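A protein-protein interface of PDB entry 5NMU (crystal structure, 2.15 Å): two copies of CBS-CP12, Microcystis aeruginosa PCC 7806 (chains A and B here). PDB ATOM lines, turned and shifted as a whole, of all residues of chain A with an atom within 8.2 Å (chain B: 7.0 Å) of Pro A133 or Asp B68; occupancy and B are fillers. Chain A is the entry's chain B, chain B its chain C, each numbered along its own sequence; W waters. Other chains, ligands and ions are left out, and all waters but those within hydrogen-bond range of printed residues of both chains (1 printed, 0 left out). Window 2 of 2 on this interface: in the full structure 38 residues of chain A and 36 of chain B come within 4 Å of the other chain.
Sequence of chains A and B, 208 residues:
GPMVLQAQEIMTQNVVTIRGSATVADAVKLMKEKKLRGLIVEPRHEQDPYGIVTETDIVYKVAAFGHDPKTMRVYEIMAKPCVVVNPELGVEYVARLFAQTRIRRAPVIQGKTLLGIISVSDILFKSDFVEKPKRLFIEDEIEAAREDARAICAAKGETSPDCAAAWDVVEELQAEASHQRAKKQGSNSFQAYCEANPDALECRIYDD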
ATOM      1  N   GLU A  92      26.606  26.759  18.814  1.00  0.00           N
ATOM      2  CA  GLU A  92      25.740  27.974  18.737  1.00  0.00           C
ATOM      3  C   GLU A  92      26.496  29.245  19.037  1.00  0.00           C
ATOM      4  O   GLU A  92      26.318  30.259  18.378  1.00  0.00           O
ATOM      5  CB  GLU A  92      24.497  27.856  19.640  1.00  0.00           C
ATOM      6  CG  GLU A  92      24.676  27.927  21.164  1.00  0.00           C
ATOM      7  CD  GLU A  92      25.049  26.620  21.810  1.00  0.00           C
ATOM      8  OE1 GLU A  92      25.927  25.902  21.313  1.00  0.00           O
ATOM      9  OE2 GLU A  92      24.453  26.272  22.836  1.00  0.00           O
ATOM     10  N   ASP A 128      24.127  20.719  14.602  1.00  0.00           N
ATOM     11  CA  ASP A 128      22.810  20.187  14.847  1.00  0.00           C
ATOM     12  C   ASP A 128      21.752  21.304  14.923  1.00  0.00           C
ATOM     13  O   ASP A 128      20.677  21.091  15.477  1.00  0.00           O
ATOM     14  CB  ASP A 128      22.837  19.325  16.141  1.00  0.00           C
ATOM     15  CG  ASP A 128      23.232  20.126  17.423  1.00  0.00           C
ATOM     16  OD1 ASP A 128      23.571  21.331  17.332  1.00  0.00           O
ATOM     17  OD2 ASP A 128      23.211  19.530  18.529  1.00  0.00           O
ATOM     18  N   PHE A 129      22.046  22.478  14.350  1.00  0.00           N
ATOM     19  CA  PHE A 129      21.175  23.670  14.472  1.00  0.00           C
ATOM     20  C   PHE A 129      19.792  23.553  13.843  1.00  0.00           C
ATOM     21  O   PHE A 129      18.910  24.361  14.160  1.00  0.00           O
ATOM     22  CB  PHE A 129      21.892  24.955  13.953  1.00  0.00           C
ATOM     23  CG  PHE A 129      22.040  25.029  12.443  1.00  0.00           C
ATOM     24  CD1 PHE A 129      23.001  24.290  11.783  1.00  0.00           C
ATOM     25  CD2 PHE A 129      21.199  25.841  11.688  1.00  0.00           C
ATOM     26  CE1 PHE A 129      23.116  24.347  10.409  1.00  0.00           C
ATOM     27  CE2 PHE A 129      21.315  25.906  10.317  1.00  0.00           C
ATOM     28  CZ  PHE A 129      22.269  25.151   9.673  1.00  0.00           C
ATOM     29  N   VAL A 130      19.599  22.583  12.945  1.00  0.00           N
ATOM     30  CA  VAL A 130      18.277  22.374  12.334  1.00  0.00           C
ATOM     31  C   VAL A 130      17.325  21.619  13.263  1.00  0.00           C
ATOM     32  O   VAL A 130      16.143  21.997  13.417  1.00  0.00           O
ATOM     33  CB  VAL A 130      18.346  21.614  10.997  1.00  0.00           C
ATOM     34  CG1 VAL A 130      16.949  21.458  10.392  1.00  0.00           C
ATOM     35  CG2 VAL A 130      19.230  22.348  10.005  1.00  0.00           C
ATOM     36  N   GLU A 131      17.821  20.537  13.846  1.00  0.00           N
ATOM     37  CA  GLU A 131      16.963  19.663  14.646  1.00  0.00           C
ATOM     38  C   GLU A 131      17.015  20.062  16.119  1.00  0.00           C
ATOM     39  O   GLU A 131      16.118  19.709  16.846  1.00  0.00           O
ATOM     40  CB  GLU A 131      17.195  18.150  14.372  1.00  0.00           C
ATOM     41  CG  GLU A 131      18.533  17.548  14.798  1.00  0.00           C
ATOM     42  CD  GLU A 131      19.708  17.825  13.851  1.00  0.00           C
ATOM     43  OE1 GLU A 131      19.554  18.626  12.889  1.00  0.00           O
ATOM     44  OE2 GLU A 131      20.800  17.241  14.094  1.00  0.00           O
ATOM     45  N   LYS A 132      18.008  20.851  16.536  1.00  0.00           N
ATOM     46  CA  LYS A 132      18.052  21.354  17.907  1.00  0.00           C
ATOM     47  C   LYS A 132      18.275  22.865  17.977  1.00  0.00           C
ATOM     48  O   LYS A 132      19.273  23.316  18.535  1.00  0.00           O
ATOM     49  CB  LYS A 132      19.166  20.658  18.685  1.00  0.00           C
ATOM     50  CG  LYS A 132      19.148  19.134  18.704  1.00  0.00           C
ATOM     51  CD  LYS A 132      20.153  18.656  19.762  1.00  0.00           C
ATOM     52  CE  LYS A 132      20.733  17.278  19.510  1.00  0.00           C
ATOM     53  NZ  LYS A 132      20.017  16.263  20.320  1.00  0.00           N
ATOM     54  N   PRO A 133      17.342  23.664  17.433  1.00  0.00           N
ATOM     55  CA  PRO A 133      17.574  25.104  17.473  1.00  0.00           C
ATOM     56  C   PRO A 133      17.762  25.582  18.908  1.00  0.00           C
ATOM     57  O   PRO A 133      16.981  25.219  19.769  1.00  0.00           O
ATOM     58  CB  PRO A 133      16.310  25.704  16.864  1.00  0.00           C
ATOM     59  CG  PRO A 133      15.460  24.577  16.394  1.00  0.00           C
ATOM     60  CD  PRO A 133      16.169  23.289  16.629  1.00  0.00           C
ATOM     61  N   LYS A 134      18.827  26.347  19.133  1.00  0.00           N
ATOM     62  CA  LYS A 134      19.276  26.789  20.472  1.00  0.00           C
ATOM     63  C   LYS A 134      18.934  28.244  20.686  1.00  0.00           C
ATOM     64  O   LYS A 134      19.657  29.113  20.223  1.00  0.00           O
ATOM     65  CB  LYS A 134      20.826  26.675  20.613  1.00  0.00           C
ATOM     66  CG  LYS A 134      21.417  25.273  20.762  1.00  0.00           C
ATOM     67  CD  LYS A 134      21.387  24.720  22.187  1.00  0.00           C
ATOM     68  CE  LYS A 134      20.131  23.912  22.470  1.00  0.00           C
ATOM     69  NZ  LYS A 134      20.033  22.639  21.704  1.00  0.00           N
ATOM     70  N   ARG A 135      17.878  28.537  21.414  1.00  0.00           N
ATOM     71  CA  ARG A 135      17.616  29.940  21.707  1.00  0.00           C
ATOM     72  C   ARG A 135      18.745  30.505  22.613  1.00  0.00           C
ATOM     73  O   ARG A 135      18.985  30.055  23.745  1.00  0.00           O
ATOM     74  CB  ARG A 135      16.250  30.094  22.319  1.00  0.00           C
ATOM     75  CG  ARG A 135      15.648  31.479  22.192  1.00  0.00           C
ATOM     76  CD  ARG A 135      14.460  31.510  23.125  1.00  0.00           C
ATOM     77  NE  ARG A 135      13.697  32.730  23.028  1.00  0.00           N
ATOM     78  CZ  ARG A 135      12.725  33.062  23.867  1.00  0.00           C
ATOM     79  NH1 ARG A 135      12.400  32.254  24.875  1.00  0.00           N
ATOM     80  NH2 ARG A 135      12.079  34.219  23.700  1.00  0.00           N
ATOM     81  N   LEU A 136      19.495  31.446  22.054  1.00  0.00           N
ATOM     82  CA  LEU A 136      20.676  31.970  22.734  1.00  0.00           C
ATOM     83  C   LEU A 136      20.177  32.728  23.976  1.00  0.00           C
ATOM     84  O   LEU A 136      19.148  33.472  23.909  1.00  0.00           O
ATOM     85  CB  LEU A 136      21.527  32.885  21.807  1.00  0.00           C
ATOM     86  CG  LEU A 136      22.754  32.312  21.063  1.00  0.00           C
ATOM     87  CD1 LEU A 136      23.870  31.905  22.015  1.00  0.00           C
ATOM     88  CD2 LEU A 136      22.395  31.140  20.168  1.00  0.00           C
ATOM     89  N   ILE A 138      18.588  31.760  26.585  1.00  0.00           N
ATOM     90  CA  ILE A 138      17.321  31.317  27.146  1.00  0.00           C
ATOM     91  C   ILE A 138      17.418  31.064  28.647  1.00  0.00           C
ATOM     92  O   ILE A 138      16.458  31.323  29.370  1.00  0.00           O
ATOM     93  CB  ILE A 138      16.764  30.084  26.385  1.00  0.00           C
ATOM     94  CG1 ILE A 138      15.320  29.796  26.812  1.00  0.00           C
ATOM     95  CG2 ILE A 138      17.642  28.841  26.565  1.00  0.00           C
ATOM     96  CD1 ILE A 138      14.565  28.920  25.827  1.00  0.00           C
ATOM     97  N   GLU A 176      10.457  24.887  27.012  1.00  0.00           N
ATOM     98  CA  GLU A 176      11.198  25.180  25.773  1.00  0.00           C
ATOM     99  C   GLU A 176      12.704  24.842  25.841  1.00  0.00           C
ATOM    100  O   GLU A 176      13.293  24.451  24.839  1.00  0.00           O
ATOM    101  CB  GLU A 176      11.003  26.655  25.408  1.00  0.00           C
ATOM    102  CG  GLU A 176      11.371  27.023  23.983  1.00  0.00           C
ATOM    103  CD  GLU A 176      11.332  28.524  23.746  1.00  0.00           C
ATOM    104  OE1 GLU A 176      10.428  29.209  24.280  1.00  0.00           O
ATOM    105  OE2 GLU A 176      12.213  29.019  23.015  1.00  0.00           O
ATOM    106  N   ALA A 177      13.327  24.998  27.007  1.00  0.00           N
ATOM    107  CA  ALA A 177      14.702  24.521  27.212  1.00  0.00           C
ATOM    108  C   ALA A 177      14.756  22.982  27.255  1.00  0.00           C
ATOM    109  O   ALA A 177      15.400  22.370  26.400  1.00  0.00           O
ATOM    110  CB  ALA A 177      15.296  25.120  28.479  1.00  0.00           C
ATOM    111  N   VAL B  24      14.403  27.300   5.283  1.00  0.00           N
ATOM    112  CA  VAL B  24      15.845  27.256   5.486  1.00  0.00           C
ATOM    113  C   VAL B  24      16.316  25.796   5.652  1.00  0.00           C
ATOM    114  O   VAL B  24      17.345  25.408   5.113  1.00  0.00           O
ATOM    115  CB  VAL B  24      16.300  28.154   6.673  1.00  0.00           C
ATOM    116  CG1 VAL B  24      17.814  28.021   6.942  1.00  0.00           C
ATOM    117  CG2 VAL B  24      15.929  29.615   6.392  1.00  0.00           C
ATOM    118  N   ALA B  25      15.552  25.005   6.397  1.00  0.00           N
ATOM    119  CA  ALA B  25      15.841  23.581   6.589  1.00  0.00           C
ATOM    120  C   ALA B  25      16.066  22.847   5.265  1.00  0.00           C
ATOM    121  O   ALA B  25      16.982  22.037   5.160  1.00  0.00           O
ATOM    122  CB  ALA B  25      14.711  22.927   7.373  1.00  0.00           C
ATOM    123  N   VAL B  62      20.652  32.625  11.245  1.00  0.00           N
ATOM    124  CA  VAL B  62      19.817  31.575  11.751  1.00  0.00           C
ATOM    125  C   VAL B  62      20.473  30.932  12.954  1.00  0.00           C
ATOM    126  O   VAL B  62      19.950  31.040  14.054  1.00  0.00           O
ATOM    127  CB  VAL B  62      19.452  30.550  10.667  1.00  0.00           C
ATOM    128  CG1 VAL B  62      18.373  29.612  11.157  1.00  0.00           C
ATOM    129  CG2 VAL B  62      18.967  31.254   9.401  1.00  0.00           C
ATOM    130  N   PHE B  65      21.516  33.042  16.147  1.00  0.00           N
ATOM    131  CA  PHE B  65      20.424  33.513  17.007  1.00  0.00           C
ATOM    132  C   PHE B  65      19.538  32.384  17.502  1.00  0.00           C
ATOM    133  O   PHE B  65      18.671  32.617  18.292  1.00  0.00           O
ATOM    134  CB  PHE B  65      19.546  34.500  16.252  1.00  0.00           C
ATOM    135  CG  PHE B  65      20.241  35.768  15.891  1.00  0.00           C
ATOM    136  CD1 PHE B  65      20.989  35.863  14.711  1.00  0.00           C
ATOM    137  CD2 PHE B  65      20.145  36.879  16.722  1.00  0.00           C
ATOM    138  CE1 PHE B  65      21.620  37.056  14.373  1.00  0.00           C
ATOM    139  CE2 PHE B  65      20.764  38.074  16.387  1.00  0.00           C
ATOM    140  CZ  PHE B  65      21.509  38.163  15.209  1.00  0.00           C
ATOM    141  N   GLY B  66      19.746  31.164  17.035  1.00  0.00           N
ATOM    142  CA  GLY B  66      18.949  30.033  17.474  1.00  0.00           C
ATOM    143  C   GLY B  66      17.573  29.927  16.852  1.00  0.00           C
ATOM    144  O   GLY B  66      16.725  29.243  17.399  1.00  0.00           O
ATOM    145  N   HIS B  67      17.366  30.579  15.707  1.00  0.00           N
ATOM    146  CA  HIS B  67      16.104  30.496  15.014  1.00  0.00           C
ATOM    147  C   HIS B  67      15.937  29.060  14.470  1.00  0.00           C
ATOM    148  O   HIS B  67      16.909  28.349  14.245  1.00  0.00           O
ATOM    149  CB  HIS B  67      15.989  31.562  13.902  1.00  0.00           C
ATOM    150  CG  HIS B  67      16.028  32.966  14.408  1.00  0.00           C
ATOM    151  ND1 HIS B  67      16.832  33.941  13.857  1.00  0.00           N
ATOM    152  CD2 HIS B  67      15.396  33.551  15.451  1.00  0.00           C
ATOM    153  CE1 HIS B  67      16.687  35.069  14.532  1.00  0.00           C
ATOM    154  NE2 HIS B  67      15.819  34.856  15.501  1.00  0.00           N
ATOM    155  N   ASP B  68      14.680  28.670  14.285  1.00  0.00           N
ATOM    156  CA  ASP B  68      14.302  27.367  13.811  1.00  0.00           C
ATOM    157  C   ASP B  68      14.351  27.388  12.300  1.00  0.00           C
ATOM    158  O   ASP B  68      13.492  28.014  11.683  1.00  0.00           O
ATOM    159  CB  ASP B  68      12.875  27.041  14.259  1.00  0.00           C
ATOM    160  CG  ASP B  68      12.488  25.608  13.956  1.00  0.00           C
ATOM    161  OD1 ASP B  68      13.189  24.928  13.164  1.00  0.00           O
ATOM    162  OD2 ASP B  68      11.498  25.152  14.541  1.00  0.00           O
ATOM    163  N   PRO B  69      15.324  26.683  11.698  1.00  0.00           N
ATOM    164  CA  PRO B  69      15.375  26.619  10.241  1.00  0.00           C
ATOM    165  C   PRO B  69      14.135  26.030   9.603  1.00  0.00           C
ATOM    166  O   PRO B  69      13.823  26.370   8.464  1.00  0.00           O
ATOM    167  CB  PRO B  69      16.559  25.694   9.976  1.00  0.00           C
ATOM    168  CG  PRO B  69      17.422  25.879  11.167  1.00  0.00           C
ATOM    169  CD  PRO B  69      16.416  25.893  12.285  1.00  0.00           C
ATOM    170  N   LYS B  70      13.437  25.161  10.331  1.00  0.00           N
ATOM    171  CA  LYS B  70      12.228  24.534   9.817  1.00  0.00           C
ATOM    172  C   LYS B  70      11.082  25.514   9.676  1.00  0.00           C
ATOM    173  O   LYS B  70      10.172  25.246   8.924  1.00  0.00           O
ATOM    174  CB  LYS B  70      11.821  23.295  10.653  1.00  0.00           C
ATOM    175  CG  LYS B  70      12.890  22.186  10.638  1.00  0.00           C
ATOM    176  CD  LYS B  70      12.522  20.910  11.416  1.00  0.00           C
ATOM    177  CE  LYS B  70      12.188  21.179  12.890  1.00  0.00           C
ATOM    178  NZ  LYS B  70      13.167  22.063  13.626  1.00  0.00           N
ATOM    179  N   THR B  71      11.110  26.637  10.385  1.00  0.00           N
ATOM    180  CA  THR B  71      10.072  27.660  10.237  1.00  0.00           C
ATOM    181  C   THR B  71      10.511  28.851   9.353  1.00  0.00           C
ATOM    182  O   THR B  71       9.668  29.488   8.738  1.00  0.00           O
ATOM    183  CB  THR B  71       9.530  28.160  11.604  1.00  0.00           C
ATOM    184  OG1 THR B  71      10.436  29.087  12.215  1.00  0.00           O
ATOM    185  CG2 THR B  71       9.278  27.011  12.542  1.00  0.00           C
ATOM    186  N   MET B  72      11.797  29.156   9.274  1.00  0.00           N
ATOM    187  CA  MET B  72      12.231  30.300   8.457  1.00  0.00           C
ATOM    188  C   MET B  72      12.260  29.955   6.989  1.00  0.00           C
ATOM    189  O   MET B  72      12.527  28.807   6.630  1.00  0.00           O
ATOM    190  CB  MET B  72      13.614  30.787   8.871  1.00  0.00           C
ATOM    191  CG  MET B  72      13.580  31.565  10.156  1.00  0.00           C
ATOM    192  SD  MET B  72      15.198  32.178  10.575  1.00  0.00           S
ATOM    193  CE  MET B  72      15.234  33.778   9.783  1.00  0.00           C
ATOM    194  N   ARG B  73      12.009  30.950   6.141  1.00  0.00           N
ATOM    195  CA  ARG B  73      12.067  30.766   4.714  1.00  0.00           C
ATOM    196  C   ARG B  73      13.272  31.479   4.122  1.00  0.00           C
ATOM    197  O   ARG B  73      13.748  32.460   4.652  1.00  0.00           O
ATOM    198  CB  ARG B  73      10.786  31.258   4.059  1.00  0.00           C
ATOM    199  CG  ARG B  73       9.497  30.657   4.601  1.00  0.00           C
ATOM    200  CD  ARG B  73       9.581  29.148   4.617  1.00  0.00           C
ATOM    201  NE  ARG B  73       8.374  28.513   5.130  1.00  0.00           N
ATOM    202  CZ  ARG B  73       7.619  27.606   4.499  1.00  0.00           C
ATOM    203  NH1 ARG B  73       7.867  27.189   3.248  1.00  0.00           N
ATOM    204  NH2 ARG B  73       6.566  27.124   5.140  1.00  0.00           N
HETATM  205  O   HOH W   1      19.274  27.222  14.620  1.00  0.00           O
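O of Val A130 lies within hydrogen-bond range of NZ of Lys B70, 3.0 Å away.
The side-chain amino group (NZ) of Lys A134 is in hydrogen-bond range of the backbone carbonyl oxygen (O) of Lys A132 (3.3 Å).
The backbone carbonyl oxygen (O) of Val B62 sits at hydrogen-bond distance from the backbone NH (N) of His B67, 3.1 Å away.
The backbone NH (N) of Val B24 sits at hydrogen-bond distance from the backbone carbonyl oxygen (O) of Pro B69, 3.4 Å away.
The backbone carbonyl oxygen (O) of Asp B68 sits at hydrogen-bond distance from the side-chain hydroxyl (OG1) of Thr B71 (3.3 Å).
N of Ala B25 lies within hydrogen-bond range of O of Pro B69 (3.0 Å).
The side-chain amino group (NZ) of Lys B70 lies within salt-bridge range of the side-chain carboxylate (OD1) of Asp B68 (2.9 Å).
Phe A129 touches Pro B69 (O to CD, 3.5 Å).
CA of Val A130 touches CG of Pro B69, 3.8 Å away.
CB of Pro A133 touches O of Gly B66 (3.6 Å).
His B67 touches Pro A133 (O to CB, 3.8 Å).
Pro A133 touches Asp B68 (CG to OD1, 3.96 Å).
Lys A134 touches Gly B66 (O to CA, 3.0 Å).
Pro A133 touches three residues of chain B.
Asp B68 touches one residue of chain A.
Pro B69 touches just these residues of chain A: Phe A129 (3.5 Å) and Val A130 (3.8 Å).
Of the printed residues of chain B, Lys A134 touches Gly B66.
Of the printed residues of chain B, Phe A129 touches Pro B69 (3.5 Å).
Arg A135 touches none of the printed residues of chain B.
The nearest residue of chain B that does not touch Pro A133 is Lys B70 (4.4 Å).
The nearest residue of chain A that does not touch Asp B68 is Val A130 (4.2 Å).
The nearest printed residue of chain B that does not touch Lys A134 is Phe B65 (4.1 Å).
Hydrophobic or aromatic side chains of chain A within 4 Å of the printed part of chain B: Phe A129 and Pro A133.
Of the 12 printed residues of chain B, 5 touch a printed residue of chain A.
Printed residues of chain B that touch a printed residue of chain A: Gly B66, His B67, Asp B68, Pro B69 and Lys B70.
Among the printed residues, 7 pairs touch across the chains.
Among the printed residues, no Asp or Glu carboxylate lies within 4 Å of a Lys or Arg side-chain nitrogen of the other chain.
No position is printed for both chains.
Water W1 lies within hydrogen-bond range of the backbone carbonyl oxygen of His B67 (2.6 Å) and the backbone carbonyl oxygen of Phe A129 (2.9 Å).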
